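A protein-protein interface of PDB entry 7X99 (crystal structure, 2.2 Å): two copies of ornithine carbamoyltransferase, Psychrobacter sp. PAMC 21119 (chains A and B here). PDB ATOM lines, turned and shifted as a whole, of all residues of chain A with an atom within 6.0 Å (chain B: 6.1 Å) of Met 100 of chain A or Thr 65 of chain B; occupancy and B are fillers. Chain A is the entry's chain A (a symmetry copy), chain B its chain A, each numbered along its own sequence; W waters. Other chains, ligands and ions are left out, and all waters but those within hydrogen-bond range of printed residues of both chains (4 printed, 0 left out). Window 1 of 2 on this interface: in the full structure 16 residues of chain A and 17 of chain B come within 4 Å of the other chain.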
ATOM      1  N   THR A  47      30.513  -5.818   2.823  1.00  0.00           N
ATOM      2  CA  THR A  47      31.585  -5.438   1.880  1.00  0.00           C
ATOM      3  C   THR A  47      32.930  -5.426   2.605  1.00  0.00           C
ATOM      4  O   THR A  47      33.016  -4.825   3.680  1.00  0.00           O
ATOM      5  CB  THR A  47      31.292  -4.091   1.218  1.00  0.00           C
ATOM      6  OG1 THR A  47      29.922  -4.041   0.807  1.00  0.00           O
ATOM      7  CG2 THR A  47      32.159  -3.859   0.001  1.00  0.00           C
ATOM      8  N   ILE A  75      35.946  -4.857  -2.432  1.00  0.00           N
ATOM      9  CA  ILE A  75      36.367  -3.696  -3.249  1.00  0.00           C
ATOM     10  C   ILE A  75      37.897  -3.652  -3.211  1.00  0.00           C
ATOM     11  O   ILE A  75      38.488  -3.514  -2.103  1.00  0.00           O
ATOM     12  CB  ILE A  75      35.793  -2.363  -2.742  1.00  0.00           C
ATOM     13  CG1 ILE A  75      34.290  -2.390  -2.455  1.00  0.00           C
ATOM     14  CG2 ILE A  75      36.157  -1.271  -3.716  1.00  0.00           C
ATOM     15  CD1 ILE A  75      33.440  -2.933  -3.566  1.00  0.00           C
ATOM     16  N   ARG A  95      38.013   6.988   7.793  1.00  0.00           N
ATOM     17  CA  ARG A  95      36.672   7.363   8.317  1.00  0.00           C
ATOM     18  C   ARG A  95      35.594   7.196   7.228  1.00  0.00           C
ATOM     19  O   ARG A  95      34.488   6.726   7.564  1.00  0.00           O
ATOM     20  CB  ARG A  95      36.714   8.800   8.839  1.00  0.00           C
ATOM     21  CG  ARG A  95      35.836   9.024  10.055  1.00  0.00           C
ATOM     22  CD  ARG A  95      35.800  10.477  10.463  1.00  0.00           C
ATOM     23  NE  ARG A  95      34.792  10.800  11.466  1.00  0.00           N
ATOM     24  CZ  ARG A  95      33.467  10.741  11.291  1.00  0.00           C
ATOM     25  NH1 ARG A  95      32.645  11.089  12.272  1.00  0.00           N
ATOM     26  NH2 ARG A  95      32.961  10.325  10.147  1.00  0.00           N
ATOM     27  N   VAL A  96      35.913   7.560   5.987  1.00  0.00           N
ATOM     28  CA  VAL A  96      34.986   7.605   4.820  1.00  0.00           C
ATOM     29  C   VAL A  96      34.818   6.180   4.273  1.00  0.00           C
ATOM     30  O   VAL A  96      33.679   5.763   4.001  1.00  0.00           O
ATOM     31  CB  VAL A  96      35.518   8.576   3.739  1.00  0.00           C
ATOM     32  CG1 VAL A  96      34.906   8.324   2.368  1.00  0.00           C
ATOM     33  CG2 VAL A  96      35.308  10.029   4.149  1.00  0.00           C
ATOM     34  N   ILE A  97      35.910   5.440   4.139  1.00  0.00           N
ATOM     35  CA  ILE A  97      35.829   4.063   3.592  1.00  0.00           C
ATOM     36  C   ILE A  97      35.076   3.186   4.589  1.00  0.00           C
ATOM     37  O   ILE A  97      34.304   2.347   4.135  1.00  0.00           O
ATOM     38  CB  ILE A  97      37.202   3.512   3.201  1.00  0.00           C
ATOM     39  CG1 ILE A  97      37.781   4.356   2.058  1.00  0.00           C
ATOM     40  CG2 ILE A  97      37.082   2.040   2.816  1.00  0.00           C
ATOM     41  CD1 ILE A  97      39.168   3.939   1.597  1.00  0.00           C
ATOM     42  N   SER A  98      35.251   3.426   5.882  1.00  0.00           N
ATOM     43  CA  SER A  98      34.658   2.600   6.942  1.00  0.00           C
ATOM     44  C   SER A  98      33.195   3.010   7.186  1.00  0.00           C
ATOM     45  O   SER A  98      32.500   2.243   7.837  1.00  0.00           O
ATOM     46  CB  SER A  98      35.508   2.624   8.175  1.00  0.00           C
ATOM     47  OG  SER A  98      35.504   3.896   8.798  1.00  0.00           O
ATOM     48  N   SER A  99      32.738   4.149   6.665  1.00  0.00           N
ATOM     49  CA  SER A  99      31.314   4.579   6.760  1.00  0.00           C
ATOM     50  C   SER A  99      30.533   3.817   5.684  1.00  0.00           C
ATOM     51  O   SER A  99      29.303   3.791   5.745  1.00  0.00           O
ATOM     52  CB  SER A  99      31.170   6.113   6.605  1.00  0.00           C
ATOM     53  OG  SER A  99      31.450   6.524   5.249  1.00  0.00           O
ATOM     54  N   MET A 100      31.238   3.271   4.689  1.00  0.00           N
ATOM     55  CA  MET A 100      30.632   2.573   3.544  1.00  0.00           C
ATOM     56  C   MET A 100      30.806   1.049   3.620  1.00  0.00           C
ATOM     57  O   MET A 100      29.863   0.366   3.239  1.00  0.00           O
ATOM     58  CB  MET A 100      31.233   3.077   2.237  1.00  0.00           C
ATOM     59  CG  MET A 100      30.457   4.237   1.726  1.00  0.00           C
ATOM     60  SD  MET A 100      31.080   4.811   0.149  1.00  0.00           S
ATOM     61  CE  MET A 100      30.692   6.538   0.400  1.00  0.00           C
ATOM     62  N   VAL A 101      31.963   0.528   4.021  1.00  0.00           N
ATOM     63  CA  VAL A 101      32.220  -0.952   3.982  1.00  0.00           C
ATOM     64  C   VAL A 101      32.145  -1.500   5.414  1.00  0.00           C
ATOM     65  O   VAL A 101      31.975  -0.708   6.324  1.00  0.00           O
ATOM     66  CB  VAL A 101      33.566  -1.269   3.299  1.00  0.00           C
ATOM     67  CG1 VAL A 101      33.640  -0.665   1.909  1.00  0.00           C
ATOM     68  CG2 VAL A 101      34.744  -0.810   4.121  1.00  0.00           C
ATOM     69  N   ASP A 102      32.254  -2.812   5.614  1.00  0.00           N
ATOM     70  CA  ASP A 102      31.986  -3.434   6.938  1.00  0.00           C
ATOM     71  C   ASP A 102      33.298  -3.908   7.579  1.00  0.00           C
ATOM     72  O   ASP A 102      33.308  -4.134   8.810  1.00  0.00           O
ATOM     73  CB  ASP A 102      30.940  -4.538   6.779  1.00  0.00           C
ATOM     74  CG  ASP A 102      29.695  -4.018   6.093  1.00  0.00           C
ATOM     75  OD1 ASP A 102      28.907  -3.363   6.776  1.00  0.00           O
ATOM     76  OD2 ASP A 102      29.550  -4.226   4.859  1.00  0.00           O
ATOM     77  N   ARG B  58      35.875   7.694  -5.513  1.00  0.00           N
ATOM     78  CA  ARG B  58      34.741   7.926  -4.574  1.00  0.00           C
ATOM     79  C   ARG B  58      33.457   7.413  -5.246  1.00  0.00           C
ATOM     80  O   ARG B  58      32.692   6.684  -4.632  1.00  0.00           O
ATOM     81  CB  ARG B  58      34.666   9.404  -4.191  1.00  0.00           C
ATOM     82  CG  ARG B  58      33.471   9.751  -3.314  1.00  0.00           C
ATOM     83  CD  ARG B  58      33.269  11.255  -3.083  1.00  0.00           C
ATOM     84  NE  ARG B  58      34.516  12.001  -2.946  1.00  0.00           N
ATOM     85  CZ  ARG B  58      35.327  11.947  -1.896  1.00  0.00           C
ATOM     86  NH1 ARG B  58      35.022  11.196  -0.846  1.00  0.00           N
ATOM     87  NH2 ARG B  58      36.442  12.666  -1.893  1.00  0.00           N
ATOM     88  N   ARG B  60      33.468   5.202  -7.700  1.00  0.00           N
ATOM     89  CA  ARG B  60      33.594   3.757  -7.982  1.00  0.00           C
ATOM     90  C   ARG B  60      33.231   2.971  -6.726  1.00  0.00           C
ATOM     91  O   ARG B  60      32.464   2.033  -6.850  1.00  0.00           O
ATOM     92  CB  ARG B  60      34.971   3.328  -8.506  1.00  0.00           C
ATOM     93  CG  ARG B  60      35.027   1.812  -8.669  1.00  0.00           C
ATOM     94  CD  ARG B  60      36.247   1.331  -9.380  1.00  0.00           C
ATOM     95  NE  ARG B  60      37.434   1.711  -8.639  1.00  0.00           N
ATOM     96  CZ  ARG B  60      37.966   1.005  -7.650  1.00  0.00           C
ATOM     97  NH1 ARG B  60      37.409  -0.132  -7.251  1.00  0.00           N
ATOM     98  NH2 ARG B  60      39.065   1.455  -7.069  1.00  0.00           N
ATOM     99  N   ILE B  61      33.806   3.313  -5.589  1.00  0.00           N
ATOM    100  CA  ILE B  61      33.630   2.548  -4.326  1.00  0.00           C
ATOM    101  C   ILE B  61      32.146   2.583  -3.953  1.00  0.00           C
ATOM    102  O   ILE B  61      31.632   1.559  -3.458  1.00  0.00           O
ATOM    103  CB  ILE B  61      34.487   3.111  -3.168  1.00  0.00           C
ATOM    104  CG1 ILE B  61      35.985   2.979  -3.437  1.00  0.00           C
ATOM    105  CG2 ILE B  61      34.125   2.463  -1.821  1.00  0.00           C
ATOM    106  CD1 ILE B  61      36.816   3.641  -2.357  1.00  0.00           C
ATOM    107  N   SER B  62      31.525   3.754  -4.055  1.00  0.00           N
ATOM    108  CA  SER B  62      30.136   3.972  -3.594  1.00  0.00           C
ATOM    109  C   SER B  62      29.180   3.150  -4.468  1.00  0.00           C
ATOM    110  O   SER B  62      28.357   2.397  -3.919  1.00  0.00           O
ATOM    111  CB  SER B  62      29.807   5.439  -3.514  1.00  0.00           C
ATOM    112  OG  SER B  62      29.967   6.050  -4.785  1.00  0.00           O
ATOM    113  N   PHE B  63      29.313   3.226  -5.779  1.00  0.00           N
ATOM    114  CA  PHE B  63      28.475   2.455  -6.731  1.00  0.00           C
ATOM    115  C   PHE B  63      28.688   0.950  -6.533  1.00  0.00           C
ATOM    116  O   PHE B  63      27.745   0.186  -6.406  1.00  0.00           O
ATOM    117  CB  PHE B  63      28.791   2.825  -8.189  1.00  0.00           C
ATOM    118  CG  PHE B  63      27.870   3.904  -8.699  1.00  0.00           C
ATOM    119  CD1 PHE B  63      26.513   3.656  -8.826  1.00  0.00           C
ATOM    120  CD2 PHE B  63      28.335   5.182  -8.927  1.00  0.00           C
ATOM    121  CE1 PHE B  63      25.653   4.661  -9.227  1.00  0.00           C
ATOM    122  CE2 PHE B  63      27.487   6.176  -9.365  1.00  0.00           C
ATOM    123  CZ  PHE B  63      26.141   5.913  -9.502  1.00  0.00           C
ATOM    124  N   GLU B  64      29.935   0.530  -6.527  1.00  0.00           N
ATOM    125  CA  GLU B  64      30.277  -0.902  -6.370  1.00  0.00           C
ATOM    126  C   GLU B  64      29.676  -1.392  -5.054  1.00  0.00           C
ATOM    127  O   GLU B  64      29.125  -2.467  -5.041  1.00  0.00           O
ATOM    128  CB  GLU B  64      31.788  -1.071  -6.431  1.00  0.00           C
ATOM    129  CG  GLU B  64      32.243  -2.326  -7.108  1.00  0.00           C
ATOM    130  CD  GLU B  64      33.759  -2.497  -7.118  1.00  0.00           C
ATOM    131  OE1 GLU B  64      34.500  -1.504  -7.394  1.00  0.00           O
ATOM    132  OE2 GLU B  64      34.191  -3.621  -6.818  1.00  0.00           O
ATOM    133  N   THR B  65      29.802  -0.622  -3.977  1.00  0.00           N
ATOM    134  CA  THR B  65      29.304  -1.057  -2.657  1.00  0.00           C
ATOM    135  C   THR B  65      27.778  -1.130  -2.739  1.00  0.00           C
ATOM    136  O   THR B  65      27.200  -2.075  -2.229  1.00  0.00           O
ATOM    137  CB  THR B  65      29.818  -0.143  -1.552  1.00  0.00           C
ATOM    138  OG1 THR B  65      31.242  -0.217  -1.571  1.00  0.00           O
ATOM    139  CG2 THR B  65      29.276  -0.511  -0.191  1.00  0.00           C
ATOM    140  N   GLY B  66      27.159  -0.164  -3.411  1.00  0.00           N
ATOM    141  CA  GLY B  66      25.698  -0.063  -3.457  1.00  0.00           C
ATOM    142  C   GLY B  66      25.098  -1.260  -4.180  1.00  0.00           C
ATOM    143  O   GLY B  66      24.188  -1.891  -3.612  1.00  0.00           O
ATOM    144  N   MET B  67      25.539  -1.523  -5.414  1.00  0.00           N
ATOM    145  CA  MET B  67      24.990  -2.609  -6.252  1.00  0.00           C
ATOM    146  C   MET B  67      25.204  -3.968  -5.550  1.00  0.00           C
ATOM    147  O   MET B  67      24.271  -4.779  -5.523  1.00  0.00           O
ATOM    148  CB  MET B  67      25.618  -2.607  -7.654  1.00  0.00           C
ATOM    149  CG  MET B  67      25.001  -3.626  -8.583  1.00  0.00           C
ATOM    150  SD  MET B  67      23.174  -3.577  -8.571  1.00  0.00           S
ATOM    151  CE  MET B  67      22.833  -3.034 -10.242  1.00  0.00           C
ATOM    152  N   GLY B  68      26.367  -4.183  -4.954  1.00  0.00           N
ATOM    153  CA  GLY B  68      26.660  -5.350  -4.109  1.00  0.00           C
ATOM    154  C   GLY B  68      25.649  -5.513  -2.978  1.00  0.00           C
ATOM    155  O   GLY B  68      25.187  -6.634  -2.767  1.00  0.00           O
ATOM    156  N   GLN B  69      25.379  -4.458  -2.208  1.00  0.00           N
ATOM    157  CA  GLN B  69      24.427  -4.530  -1.064  1.00  0.00           C
ATOM    158  C   GLN B  69      23.057  -4.949  -1.593  1.00  0.00           C
ATOM    159  O   GLN B  69      22.350  -5.682  -0.879  1.00  0.00           O
ATOM    160  CB  GLN B  69      24.347  -3.206  -0.316  1.00  0.00           C
ATOM    161  CG  GLN B  69      25.542  -2.984   0.596  1.00  0.00           C
ATOM    162  CD  GLN B  69      25.514  -1.599   1.196  1.00  0.00           C
ATOM    163  OE1 GLN B  69      24.681  -0.759   0.855  1.00  0.00           O
ATOM    164  NE2 GLN B  69      26.459  -1.342   2.070  1.00  0.00           N
ATOM    165  N   PHE B  70      22.727  -4.552  -2.819  1.00  0.00           N
ATOM    166  CA  PHE B  70      21.424  -4.871  -3.457  1.00  0.00           C
ATOM    167  C   PHE B  70      21.411  -6.253  -4.085  1.00  0.00           C
ATOM    168  O   PHE B  70      20.376  -6.610  -4.650  1.00  0.00           O
ATOM    169  CB  PHE B  70      21.095  -3.875  -4.559  1.00  0.00           C
ATOM    170  CG  PHE B  70      20.427  -2.587  -4.152  1.00  0.00           C
ATOM    171  CD1 PHE B  70      19.668  -2.483  -3.014  1.00  0.00           C
ATOM    172  CD2 PHE B  70      20.475  -1.499  -5.002  1.00  0.00           C
ATOM    173  CE1 PHE B  70      18.971  -1.315  -2.732  1.00  0.00           C
ATOM    174  CE2 PHE B  70      19.810  -0.317  -4.705  1.00  0.00           C
ATOM    175  CZ  PHE B  70      19.050  -0.231  -3.575  1.00  0.00           C
ATOM    176  N   ALA B 287      29.838  12.425   2.340  1.00  0.00           N
ATOM    177  CA  ALA B 287      30.651  11.340   1.726  1.00  0.00           C
ATOM    178  C   ALA B 287      29.918   9.991   1.821  1.00  0.00           C
ATOM    179  O   ALA B 287      29.857   9.266   0.813  1.00  0.00           O
ATOM    180  CB  ALA B 287      32.004  11.249   2.383  1.00  0.00           C
ATOM    181  N   GLU B 288      29.362   9.654   2.985  1.00  0.00           N
ATOM    182  CA  GLU B 288      28.735   8.326   3.169  1.00  0.00           C
ATOM    183  C   GLU B 288      27.507   8.255   2.245  1.00  0.00           C
ATOM    184  O   GLU B 288      27.295   7.259   1.596  1.00  0.00           O
ATOM    185  CB  GLU B 288      28.331   8.130   4.623  1.00  0.00           C
ATOM    186  CG  GLU B 288      27.697   6.773   4.799  1.00  0.00           C
ATOM    187  CD  GLU B 288      27.207   6.393   6.170  1.00  0.00           C
ATOM    188  OE1 GLU B 288      27.725   6.975   7.166  1.00  0.00           O
ATOM    189  OE2 GLU B 288      26.335   5.446   6.217  1.00  0.00           O
ATOM    190  N   ASN B 289      26.738   9.329   2.167  1.00  0.00           N
ATOM    191  CA  ASN B 289      25.441   9.330   1.456  1.00  0.00           C
ATOM    192  C   ASN B 289      25.586   9.217  -0.073  1.00  0.00           C
ATOM    193  O   ASN B 289      24.548   8.971  -0.728  1.00  0.00           O
ATOM    194  CB  ASN B 289      24.620  10.541   1.866  1.00  0.00           C
ATOM    195  CG  ASN B 289      24.018  10.322   3.241  1.00  0.00           C
ATOM    196  OD1 ASN B 289      23.935   9.192   3.700  1.00  0.00           O
ATOM    197  ND2 ASN B 289      23.612  11.391   3.899  1.00  0.00           N
ATOM    198  N   ARG B 290      26.778   9.339  -0.654  1.00  0.00           N
ATOM    199  CA  ARG B 290      26.967   8.884  -2.066  1.00  0.00           C
ATOM    200  C   ARG B 290      26.489   7.434  -2.178  1.00  0.00           C
ATOM    201  O   ARG B 290      25.865   7.060  -3.181  1.00  0.00           O
ATOM    202  CB  ARG B 290      28.423   8.974  -2.525  1.00  0.00           C
ATOM    203  CG  ARG B 290      28.936  10.385  -2.679  1.00  0.00           C
ATOM    204  CD  ARG B 290      28.215  11.092  -3.813  1.00  0.00           C
ATOM    205  NE  ARG B 290      28.526  10.438  -5.057  1.00  0.00           N
ATOM    206  CZ  ARG B 290      29.611  10.680  -5.817  1.00  0.00           C
ATOM    207  NH1 ARG B 290      30.522  11.584  -5.475  1.00  0.00           N
ATOM    208  NH2 ARG B 290      29.756  10.011  -6.939  1.00  0.00           N
ATOM    209  N   LEU B 291      26.757   6.628  -1.168  1.00  0.00           N
ATOM    210  CA  LEU B 291      26.335   5.203  -1.195  1.00  0.00           C
ATOM    211  C   LEU B 291      24.811   5.127  -1.279  1.00  0.00           C
ATOM    212  O   LEU B 291      24.292   4.513  -2.212  1.00  0.00           O
ATOM    213  CB  LEU B 291      26.863   4.521   0.055  1.00  0.00           C
ATOM    214  CG  LEU B 291      26.300   3.129   0.305  1.00  0.00           C
ATOM    215  CD1 LEU B 291      26.490   2.240  -0.905  1.00  0.00           C
ATOM    216  CD2 LEU B 291      26.967   2.537   1.528  1.00  0.00           C
ATOM    217  N   LYS B 295      22.131   4.281  -4.365  1.00  0.00           N
ATOM    218  CA  LYS B 295      21.227   3.103  -4.264  1.00  0.00           C
ATOM    219  C   LYS B 295      19.792   3.535  -4.565  1.00  0.00           C
ATOM    220  O   LYS B 295      19.184   2.897  -5.431  1.00  0.00           O
ATOM    221  CB  LYS B 295      21.365   2.443  -2.903  1.00  0.00           C
ATOM    222  CG  LYS B 295      22.658   1.669  -2.733  1.00  0.00           C
ATOM    223  CD  LYS B 295      22.786   1.104  -1.311  1.00  0.00           C
ATOM    224  CE  LYS B 295      21.882  -0.105  -1.106  1.00  0.00           C
ATOM    225  NZ  LYS B 295      21.965  -0.565   0.298  1.00  0.00           N
HETATM  226  O   HOH W   1      28.187  -3.434   2.712  1.00  0.00           O
HETATM  227  O   HOH W   2      26.629   2.861   5.447  1.00  0.00           O
HETATM  228  O   HOH W   3      28.689  -4.448  -1.466  1.00  0.00           O
HETATM  229  O   HOH W   4      27.161   0.404   4.188  1.00  0.00           O
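OE2 of Glu 288 of chain B lies close to O of Ser 99 of chain A, at 3.4 Å.
The side-chain hydroxyl (OG) of Ser 62 of chain B lies within hydrogen-bond range of the backbone carbonyl oxygen (O) of Arg 58 of chain B, 2.8 Å away.
The guanidinium group of Arg 60 of chain B is in salt-bridge range of the side-chain carboxylate of Glu 64 of chain B, at 3.2 Å.
OG1 of Thr 65 of chain B sits at hydrogen-bond distance from O of Ile 61 of chain B (2.6 Å).
The side-chain amide oxygen (OE1) of Gln 69 of chain B sits at hydrogen-bond distance from the side-chain amino group (NZ) of Lys 295 of chain B (2.8 Å).
N of Thr 47 of chain A sits at hydrogen-bond distance from OD2 of Asp 102 of chain A, 2.8 Å away.
O of Val 96 of chain A sits at hydrogen-bond distance from OG of Ser 99 of chain A, at 2.7 Å.
Thr 65 of chain B touches Thr 47 of chain A.
Ile 75 of chain A touches Arg 60 of chain B.
Ile 75 of chain A touches Glu 64 of chain B (CD1 to OE2, 3.4 Å).
CG1 of Ile 75 of chain A touches OG1 of Thr 65 of chain B (3.8 Å).
CG2 of Val 96 of chain A touches CB of Ala 287 of chain B, at 3.9 Å.
CG2 of Thr 65 of chain B touches O of Met 100 of chain A (3.6 Å).
Met 100 of chain A touches Gln 69 of chain B.
Met 100 of chain A touches Ala 287 of chain B (CE to O, 2.9 Å).
Glu 288 of chain B touches Met 100 of chain A (O to CE, 3.7 Å).
CG of Met 100 of chain A touches CD2 of Leu 291 of chain B (3.9 Å).
Of the printed residues of chain B, Ser 99 of chain A touches Glu 288.
Of the printed residues of chain A, Arg 60 of chain B touches Ile 75 (3.9 Å).
Of the printed residues of chain A, Ser 62 of chain B touches Met 100.
Of chain A, only Thr 47 (3.7 Å), Ile 75 (3.8 Å) and Met 100 (3.6 Å) come within 4 Å of Thr 65 of chain B.
The nearest printed residue of chain B that does not touch Met 100 of chain A is Ile 61 of chain B (4.3 Å).
The nearest residue of chain A that does not touch Thr 65 of chain B is Val 101 of chain A (4.2 Å).
Printed residues of chain B that touch a printed residue of chain A: Arg 60, Ser 62, Glu 64, Thr 65, Gln 69, Ala 287, Glu 288 and Leu 291.
Hydrophobic or aromatic side chains of chain B within 4 Å of the printed part of chain A: Ala 287 and Leu 291.
Along chain A the printed residues that touch a printed residue of chain B span positions 47 to 100.
Among the printed residues, no Asp or Glu carboxylate lies within 4 Å of a Lys or Arg side-chain nitrogen of the other chain.
No position is printed for both chains.
Water W3 lies within hydrogen-bond range of OG1 of Thr 47 of chain A (2.6 Å), O of Thr 65 of chain B (2.9 Å) and N of Gln 69 of chain B (3.4 Å).
Water W1 lies within hydrogen-bond range of OG1 of Thr 47 of chain A (2.6 Å), OD2 of Asp 102 of chain A (2.7 Å) and NE2 of Gln 69 of chain B (2.8 Å).
Water W2 lies within hydrogen-bond range of OE2 of Glu 288 of chain B (2.7 Å) and O of Ser 99 of chain A (2.8 Å).
Water W4 bridges the side-chain amide nitrogen (NE2) of Gln 69 of chain B and the backbone carbonyl oxygen (O) of Met 100 of chain A.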
